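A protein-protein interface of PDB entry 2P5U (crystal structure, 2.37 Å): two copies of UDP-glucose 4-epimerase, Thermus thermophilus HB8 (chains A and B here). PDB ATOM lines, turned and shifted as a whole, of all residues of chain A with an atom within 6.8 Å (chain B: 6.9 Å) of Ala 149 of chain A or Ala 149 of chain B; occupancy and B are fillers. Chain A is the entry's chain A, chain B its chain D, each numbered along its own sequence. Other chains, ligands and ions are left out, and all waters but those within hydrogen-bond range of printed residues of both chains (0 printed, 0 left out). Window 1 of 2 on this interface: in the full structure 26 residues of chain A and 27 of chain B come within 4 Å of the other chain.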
ATOM      1  N   LEU A  94     -22.064  10.697  32.371  1.00  0.00           N
ATOM      2  CA  LEU A  94     -21.336  11.075  31.161  1.00  0.00           C
ATOM      3  C   LEU A  94     -20.276  12.135  31.434  1.00  0.00           C
ATOM      4  O   LEU A  94     -19.083  11.895  31.253  1.00  0.00           O
ATOM      5  CB  LEU A  94     -22.287  11.605  30.082  1.00  0.00           C
ATOM      6  CG  LEU A  94     -22.642  10.697  28.907  1.00  0.00           C
ATOM      7  CD1 LEU A  94     -21.420   9.855  28.535  1.00  0.00           C
ATOM      8  CD2 LEU A  94     -23.796   9.808  29.265  1.00  0.00           C
ATOM      9  N   ALA A 144     -29.867   3.919  31.340  1.00  0.00           N
ATOM     10  CA  ALA A 144     -29.300   2.920  30.450  1.00  0.00           C
ATOM     11  C   ALA A 144     -28.583   3.590  29.274  1.00  0.00           C
ATOM     12  O   ALA A 144     -27.607   3.048  28.754  1.00  0.00           O
ATOM     13  CB  ALA A 144     -30.400   1.980  29.935  1.00  0.00           C
ATOM     14  N   ALA A 145     -29.060   4.762  28.855  1.00  0.00           N
ATOM     15  CA  ALA A 145     -28.429   5.471  27.742  1.00  0.00           C
ATOM     16  C   ALA A 145     -27.076   6.036  28.148  1.00  0.00           C
ATOM     17  O   ALA A 145     -26.123   6.008  27.366  1.00  0.00           O
ATOM     18  CB  ALA A 145     -29.334   6.601  27.230  1.00  0.00           C
ATOM     19  N   SER A 146     -26.971   6.538  29.372  1.00  0.00           N
ATOM     20  CA  SER A 146     -25.697   7.092  29.810  1.00  0.00           C
ATOM     21  C   SER A 146     -24.664   5.969  29.948  1.00  0.00           C
ATOM     22  O   SER A 146     -23.477   6.159  29.674  1.00  0.00           O
ATOM     23  CB  SER A 146     -25.861   7.829  31.139  1.00  0.00           C
ATOM     24  OG  SER A 146     -26.217   6.936  32.173  1.00  0.00           O
ATOM     25  N   LYS A 147     -25.113   4.791  30.356  1.00  0.00           N
ATOM     26  CA  LYS A 147     -24.194   3.667  30.503  1.00  0.00           C
ATOM     27  C   LYS A 147     -23.746   3.159  29.122  1.00  0.00           C
ATOM     28  O   LYS A 147     -22.564   2.866  28.909  1.00  0.00           O
ATOM     29  CB  LYS A 147     -24.868   2.542  31.284  1.00  0.00           C
ATOM     30  CG  LYS A 147     -24.258   2.269  32.654  1.00  0.00           C
ATOM     31  CD  LYS A 147     -24.335   3.452  33.586  1.00  0.00           C
ATOM     32  CE  LYS A 147     -24.172   3.005  35.036  1.00  0.00           C
ATOM     33  NZ  LYS A 147     -22.773   2.845  35.502  1.00  0.00           N
ATOM     34  N   ALA A 148     -24.688   3.051  28.190  1.00  0.00           N
ATOM     35  CA  ALA A 148     -24.354   2.590  26.851  1.00  0.00           C
ATOM     36  C   ALA A 148     -23.417   3.607  26.185  1.00  0.00           C
ATOM     37  O   ALA A 148     -22.487   3.236  25.481  1.00  0.00           O
ATOM     38  CB  ALA A 148     -25.629   2.414  26.021  1.00  0.00           C
ATOM     39  N   ALA A 149     -23.671   4.888  26.425  1.00  0.00           N
ATOM     40  CA  ALA A 149     -22.861   5.954  25.858  1.00  0.00           C
ATOM     41  C   ALA A 149     -21.448   5.901  26.416  1.00  0.00           C
ATOM     42  O   ALA A 149     -20.472   6.104  25.688  1.00  0.00           O
ATOM     43  CB  ALA A 149     -23.483   7.319  26.158  1.00  0.00           C
ATOM     44  N   PHE A 150     -21.323   5.637  27.709  1.00  0.00           N
ATOM     45  CA  PHE A 150     -19.990   5.584  28.280  1.00  0.00           C
ATOM     46  C   PHE A 150     -19.194   4.397  27.716  1.00  0.00           C
ATOM     47  O   PHE A 150     -17.979   4.498  27.541  1.00  0.00           O
ATOM     48  CB  PHE A 150     -20.042   5.504  29.808  1.00  0.00           C
ATOM     49  CG  PHE A 150     -18.703   5.705  30.451  1.00  0.00           C
ATOM     50  CD1 PHE A 150     -18.130   6.973  30.511  1.00  0.00           C
ATOM     51  CD2 PHE A 150     -17.978   4.620  30.928  1.00  0.00           C
ATOM     52  CE1 PHE A 150     -16.849   7.154  31.034  1.00  0.00           C
ATOM     53  CE2 PHE A 150     -16.700   4.787  31.450  1.00  0.00           C
ATOM     54  CZ  PHE A 150     -16.135   6.058  31.503  1.00  0.00           C
ATOM     55  N   GLU A 151     -19.871   3.277  27.442  1.00  0.00           N
ATOM     56  CA  GLU A 151     -19.190   2.110  26.887  1.00  0.00           C
ATOM     57  C   GLU A 151     -18.610   2.509  25.528  1.00  0.00           C
ATOM     58  O   GLU A 151     -17.503   2.115  25.171  1.00  0.00           O
ATOM     59  CB  GLU A 151     -20.151   0.916  26.702  1.00  0.00           C
ATOM     60  CG  GLU A 151     -20.629   0.248  27.997  1.00  0.00           C
ATOM     61  CD  GLU A 151     -21.446  -1.030  27.758  1.00  0.00           C
ATOM     62  OE1 GLU A 151     -22.132  -1.127  26.716  1.00  0.00           O
ATOM     63  OE2 GLU A 151     -21.421  -1.930  28.622  1.00  0.00           O
ATOM     64  N   HIS A 152     -19.354   3.301  24.770  1.00  0.00           N
ATOM     65  CA  HIS A 152     -18.865   3.723  23.466  1.00  0.00           C
ATOM     66  C   HIS A 152     -17.600   4.558  23.602  1.00  0.00           C
ATOM     67  O   HIS A 152     -16.665   4.377  22.831  1.00  0.00           O
ATOM     68  CB  HIS A 152     -19.956   4.494  22.710  1.00  0.00           C
ATOM     69  CG  HIS A 152     -20.989   3.610  22.093  1.00  0.00           C
ATOM     70  ND1 HIS A 152     -22.328   3.944  22.031  1.00  0.00           N
ATOM     71  CD2 HIS A 152     -20.868   2.414  21.470  1.00  0.00           C
ATOM     72  CE1 HIS A 152     -22.982   2.989  21.394  1.00  0.00           C
ATOM     73  NE2 HIS A 152     -22.119   2.052  21.042  1.00  0.00           N
ATOM     74  N   TYR A 153     -17.567   5.464  24.579  1.00  0.00           N
ATOM     75  CA  TYR A 153     -16.385   6.298  24.778  1.00  0.00           C
ATOM     76  C   TYR A 153     -15.149   5.493  25.148  1.00  0.00           C
ATOM     77  O   TYR A 153     -14.067   5.724  24.611  1.00  0.00           O
ATOM     78  CB  TYR A 153     -16.625   7.384  25.844  1.00  0.00           C
ATOM     79  CG  TYR A 153     -17.233   8.642  25.265  1.00  0.00           C
ATOM     80  CD1 TYR A 153     -18.620   8.828  25.235  1.00  0.00           C
ATOM     81  CD2 TYR A 153     -16.429   9.592  24.635  1.00  0.00           C
ATOM     82  CE1 TYR A 153     -19.190   9.927  24.574  1.00  0.00           C
ATOM     83  CE2 TYR A 153     -16.986  10.686  23.976  1.00  0.00           C
ATOM     84  CZ  TYR A 153     -18.357  10.847  23.943  1.00  0.00           C
ATOM     85  OH  TYR A 153     -18.873  11.914  23.244  1.00  0.00           O
ATOM     86  N   LEU A 154     -15.282   4.534  26.052  1.00  0.00           N
ATOM     87  CA  LEU A 154     -14.090   3.789  26.401  1.00  0.00           C
ATOM     88  C   LEU A 154     -13.646   2.918  25.230  1.00  0.00           C
ATOM     89  O   LEU A 154     -12.466   2.598  25.101  1.00  0.00           O
ATOM     90  CB  LEU A 154     -14.306   2.994  27.695  1.00  0.00           C
ATOM     91  CG  LEU A 154     -15.624   2.269  27.868  1.00  0.00           C
ATOM     92  CD1 LEU A 154     -15.568   1.032  27.002  1.00  0.00           C
ATOM     93  CD2 LEU A 154     -15.853   1.891  29.334  1.00  0.00           C
ATOM     94  N   LEU B  94     -22.956  16.161  22.763  1.00  0.00           N
ATOM     95  CA  LEU B  94     -23.758  15.511  23.791  1.00  0.00           C
ATOM     96  C   LEU B  94     -24.334  16.493  24.796  1.00  0.00           C
ATOM     97  O   LEU B  94     -25.543  16.512  25.017  1.00  0.00           O
ATOM     98  CB  LEU B  94     -22.944  14.453  24.528  1.00  0.00           C
ATOM     99  CG  LEU B  94     -22.999  13.071  23.897  1.00  0.00           C
ATOM    100  CD1 LEU B  94     -22.154  12.108  24.713  1.00  0.00           C
ATOM    101  CD2 LEU B  94     -24.453  12.600  23.831  1.00  0.00           C
ATOM    102  N   TYR B 143     -15.980  11.501  18.098  1.00  0.00           N
ATOM    103  CA  TYR B 143     -17.053  12.077  17.304  1.00  0.00           C
ATOM    104  C   TYR B 143     -18.107  11.021  17.004  1.00  0.00           C
ATOM    105  O   TYR B 143     -19.303  11.259  17.167  1.00  0.00           O
ATOM    106  CB  TYR B 143     -16.482  12.633  16.004  1.00  0.00           C
ATOM    107  CG  TYR B 143     -17.508  12.881  14.932  1.00  0.00           C
ATOM    108  CD1 TYR B 143     -17.711  11.952  13.907  1.00  0.00           C
ATOM    109  CD2 TYR B 143     -18.235  14.078  14.903  1.00  0.00           C
ATOM    110  CE1 TYR B 143     -18.600  12.217  12.871  1.00  0.00           C
ATOM    111  CE2 TYR B 143     -19.125  14.350  13.871  1.00  0.00           C
ATOM    112  CZ  TYR B 143     -19.295  13.417  12.856  1.00  0.00           C
ATOM    113  OH  TYR B 143     -20.112  13.715  11.790  1.00  0.00           O
ATOM    114  N   ALA B 144     -17.662   9.854  16.559  1.00  0.00           N
ATOM    115  CA  ALA B 144     -18.594   8.771  16.250  1.00  0.00           C
ATOM    116  C   ALA B 144     -19.270   8.291  17.536  1.00  0.00           C
ATOM    117  O   ALA B 144     -20.443   7.924  17.525  1.00  0.00           O
ATOM    118  CB  ALA B 144     -17.855   7.605  15.573  1.00  0.00           C
ATOM    119  N   ALA B 145     -18.527   8.291  18.641  1.00  0.00           N
ATOM    120  CA  ALA B 145     -19.098   7.857  19.912  1.00  0.00           C
ATOM    121  C   ALA B 145     -20.167   8.862  20.348  1.00  0.00           C
ATOM    122  O   ALA B 145     -21.205   8.498  20.911  1.00  0.00           O
ATOM    123  CB  ALA B 145     -18.004   7.743  20.983  1.00  0.00           C
ATOM    124  N   SER B 146     -19.899  10.132  20.069  1.00  0.00           N
ATOM    125  CA  SER B 146     -20.802  11.227  20.405  1.00  0.00           C
ATOM    126  C   SER B 146     -22.131  11.072  19.661  1.00  0.00           C
ATOM    127  O   SER B 146     -23.218  11.231  20.233  1.00  0.00           O
ATOM    128  CB  SER B 146     -20.149  12.551  20.010  1.00  0.00           C
ATOM    129  OG  SER B 146     -20.720  13.625  20.727  1.00  0.00           O
ATOM    130  N   LYS B 147     -22.029  10.762  18.374  1.00  0.00           N
ATOM    131  CA  LYS B 147     -23.205  10.581  17.526  1.00  0.00           C
ATOM    132  C   LYS B 147     -24.012   9.343  17.917  1.00  0.00           C
ATOM    133  O   LYS B 147     -25.244   9.382  17.954  1.00  0.00           O
ATOM    134  CB  LYS B 147     -22.772  10.474  16.063  1.00  0.00           C
ATOM    135  CG  LYS B 147     -22.239  11.771  15.489  1.00  0.00           C
ATOM    136  CD  LYS B 147     -23.347  12.807  15.378  1.00  0.00           C
ATOM    137  CE  LYS B 147     -22.834  14.112  14.752  1.00  0.00           C
ATOM    138  NZ  LYS B 147     -23.952  15.030  14.410  1.00  0.00           N
ATOM    139  N   ALA B 148     -23.315   8.249  18.206  1.00  0.00           N
ATOM    140  CA  ALA B 148     -23.976   7.015  18.590  1.00  0.00           C
ATOM    141  C   ALA B 148     -24.662   7.211  19.939  1.00  0.00           C
ATOM    142  O   ALA B 148     -25.781   6.742  20.152  1.00  0.00           O
ATOM    143  CB  ALA B 148     -22.960   5.872  18.667  1.00  0.00           C
ATOM    144  N   ALA B 149     -23.990   7.905  20.849  1.00  0.00           N
ATOM    145  CA  ALA B 149     -24.566   8.165  22.167  1.00  0.00           C
ATOM    146  C   ALA B 149     -25.842   8.999  22.041  1.00  0.00           C
ATOM    147  O   ALA B 149     -26.846   8.693  22.678  1.00  0.00           O
ATOM    148  CB  ALA B 149     -23.553   8.884  23.057  1.00  0.00           C
ATOM    149  N   PHE B 150     -25.825  10.036  21.207  1.00  0.00           N
ATOM    150  CA  PHE B 150     -27.016  10.864  21.070  1.00  0.00           C
ATOM    151  C   PHE B 150     -28.205  10.065  20.520  1.00  0.00           C
ATOM    152  O   PHE B 150     -29.355  10.338  20.873  1.00  0.00           O
ATOM    153  CB  PHE B 150     -26.729  12.090  20.195  1.00  0.00           C
ATOM    154  CG  PHE B 150     -27.806  13.139  20.262  1.00  0.00           C
ATOM    155  CD1 PHE B 150     -28.693  13.313  19.203  1.00  0.00           C
ATOM    156  CD2 PHE B 150     -27.962  13.923  21.410  1.00  0.00           C
ATOM    157  CE1 PHE B 150     -29.726  14.252  19.281  1.00  0.00           C
ATOM    158  CE2 PHE B 150     -28.989  14.863  21.505  1.00  0.00           C
ATOM    159  CZ  PHE B 150     -29.876  15.028  20.437  1.00  0.00           C
ATOM    160  N   GLU B 151     -27.927   9.084  19.665  1.00  0.00           N
ATOM    161  CA  GLU B 151     -28.982   8.236  19.116  1.00  0.00           C
ATOM    162  C   GLU B 151     -29.639   7.480  20.273  1.00  0.00           C
ATOM    163  O   GLU B 151     -30.852   7.254  20.275  1.00  0.00           O
ATOM    164  CB  GLU B 151     -28.417   7.226  18.099  1.00  0.00           C
ATOM    165  CG  GLU B 151     -28.126   7.814  16.718  1.00  0.00           C
ATOM    166  CD  GLU B 151     -27.637   6.783  15.691  1.00  0.00           C
ATOM    167  OE1 GLU B 151     -27.627   7.111  14.481  1.00  0.00           O
ATOM    168  OE2 GLU B 151     -27.260   5.655  16.090  1.00  0.00           O
ATOM    169  N   HIS B 152     -28.842   7.073  21.258  1.00  0.00           N
ATOM    170  CA  HIS B 152     -29.422   6.365  22.389  1.00  0.00           C
ATOM    171  C   HIS B 152     -30.348   7.293  23.153  1.00  0.00           C
ATOM    172  O   HIS B 152     -31.446   6.898  23.544  1.00  0.00           O
ATOM    173  CB  HIS B 152     -28.335   5.824  23.309  1.00  0.00           C
ATOM    174  CG  HIS B 152     -27.582   4.683  22.711  1.00  0.00           C
ATOM    175  ND1 HIS B 152     -26.205   4.602  22.730  1.00  0.00           N
ATOM    176  CD2 HIS B 152     -28.017   3.582  22.055  1.00  0.00           C
ATOM    177  CE1 HIS B 152     -25.827   3.500  22.109  1.00  0.00           C
ATOM    178  NE2 HIS B 152     -26.904   2.863  21.689  1.00  0.00           N
ATOM    179  N   TYR B 153     -29.918   8.532  23.345  1.00  0.00           N
ATOM    180  CA  TYR B 153     -30.748   9.484  24.056  1.00  0.00           C
ATOM    181  C   TYR B 153     -32.052   9.750  23.307  1.00  0.00           C
ATOM    182  O   TYR B 153     -33.126   9.812  23.915  1.00  0.00           O
ATOM    183  CB  TYR B 153     -29.949  10.759  24.314  1.00  0.00           C
ATOM    184  CG  TYR B 153     -29.189  10.664  25.623  1.00  0.00           C
ATOM    185  CD1 TYR B 153     -29.841  10.863  26.842  1.00  0.00           C
ATOM    186  CD2 TYR B 153     -27.837  10.326  25.649  1.00  0.00           C
ATOM    187  CE1 TYR B 153     -29.167  10.733  28.050  1.00  0.00           C
ATOM    188  CE2 TYR B 153     -27.155  10.189  26.859  1.00  0.00           C
ATOM    189  CZ  TYR B 153     -27.828  10.397  28.049  1.00  0.00           C
ATOM    190  OH  TYR B 153     -27.159  10.302  29.237  1.00  0.00           O
ATOM    191  N   LEU B 154     -31.972   9.882  21.986  1.00  0.00           N
ATOM    192  CA  LEU B 154     -33.184  10.095  21.205  1.00  0.00           C
ATOM    193  C   LEU B 154     -34.159   8.940  21.446  1.00  0.00           C
ATOM    194  O   LEU B 154     -35.341   9.162  21.687  1.00  0.00           O
ATOM    195  CB  LEU B 154     -32.862  10.176  19.714  1.00  0.00           C
ATOM    196  CG  LEU B 154     -32.307  11.497  19.199  1.00  0.00           C
ATOM    197  CD1 LEU B 154     -31.695  11.276  17.820  1.00  0.00           C
ATOM    198  CD2 LEU B 154     -33.426  12.544  19.147  1.00  0.00           C
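O of Ala 148 of chain B sits at hydrogen-bond distance from ND1 of His 152 of chain B (3.4 Å).
Leu 94 of chain A touches Tyr 153 of chain B (CD2 to OH, 3.4 Å). Tyr 153 of chain B touches Ser 146 of chain A. His 152 of chain B touches Ala 148 of chain A. Ala 149 of chain B touches Ala 149 of chain A. His 152 of chain A touches Ala 148 of chain B. His 152 of chain B touches His 152 of chain A (CE1 to CE1, 3.0 Å). Tyr 153 of chain A touches Leu 94 of chain B (OH to CD1, 3.6 Å). CA of Ser 146 of chain B touches OH of Tyr 153 of chain A, at 3.5 Å.
Of the printed residues of chain B, Ala 149 of chain A touches Ala 149 (3.5 Å). Printed residues of chain A within 4 Å of Ala 149 of chain B: Ala 149. Printed residues of chain B within 4 Å of Leu 94 of chain A: Tyr 153 (3.4 Å). Printed residues of chain A within 4 Å of Ala 148 of chain B: His 152 (3.9 Å). Printed residues of chain B within 4 Å of Ala 148 of chain A: His 152. Of the printed residues of chain A, Tyr 153 of chain B touches Leu 94 (3.4 Å) and Ser 146 (3.4 Å). Phe 150 of chain A touches none of the printed residues of chain B. Ala 145 of chain A touches none of the printed residues of chain B. The nearest residue of chain B that does not touch Ala 149 of chain A is His 152 of chain B (4.5 Å).
Of the 13 printed residues of chain B, 6 touch a printed residue of chain A. Among the printed residues, 8 pairs touch across the chains.
Leu 94 of chain A touches Tyr 153 of chain B, and with the chains exchanged Tyr 153 of chain A touches Leu 94 of chain B. Ser 146 of chain A touches Tyr 153 of chain B, and with the chains exchanged Tyr 153 of chain A touches Ser 146 of chain B. Ala 148 of chain A touches His 152 of chain B, and with the chains exchanged His 152 of chain A touches Ala 148 of chain B. His 152 of chain A touches its own counterpart, His 152 of chain B. 12 positions are printed for both chains. Of the 8 pairs that touch across the chains among the printed residues, 8 have their exchanged pair printed and touching as well.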
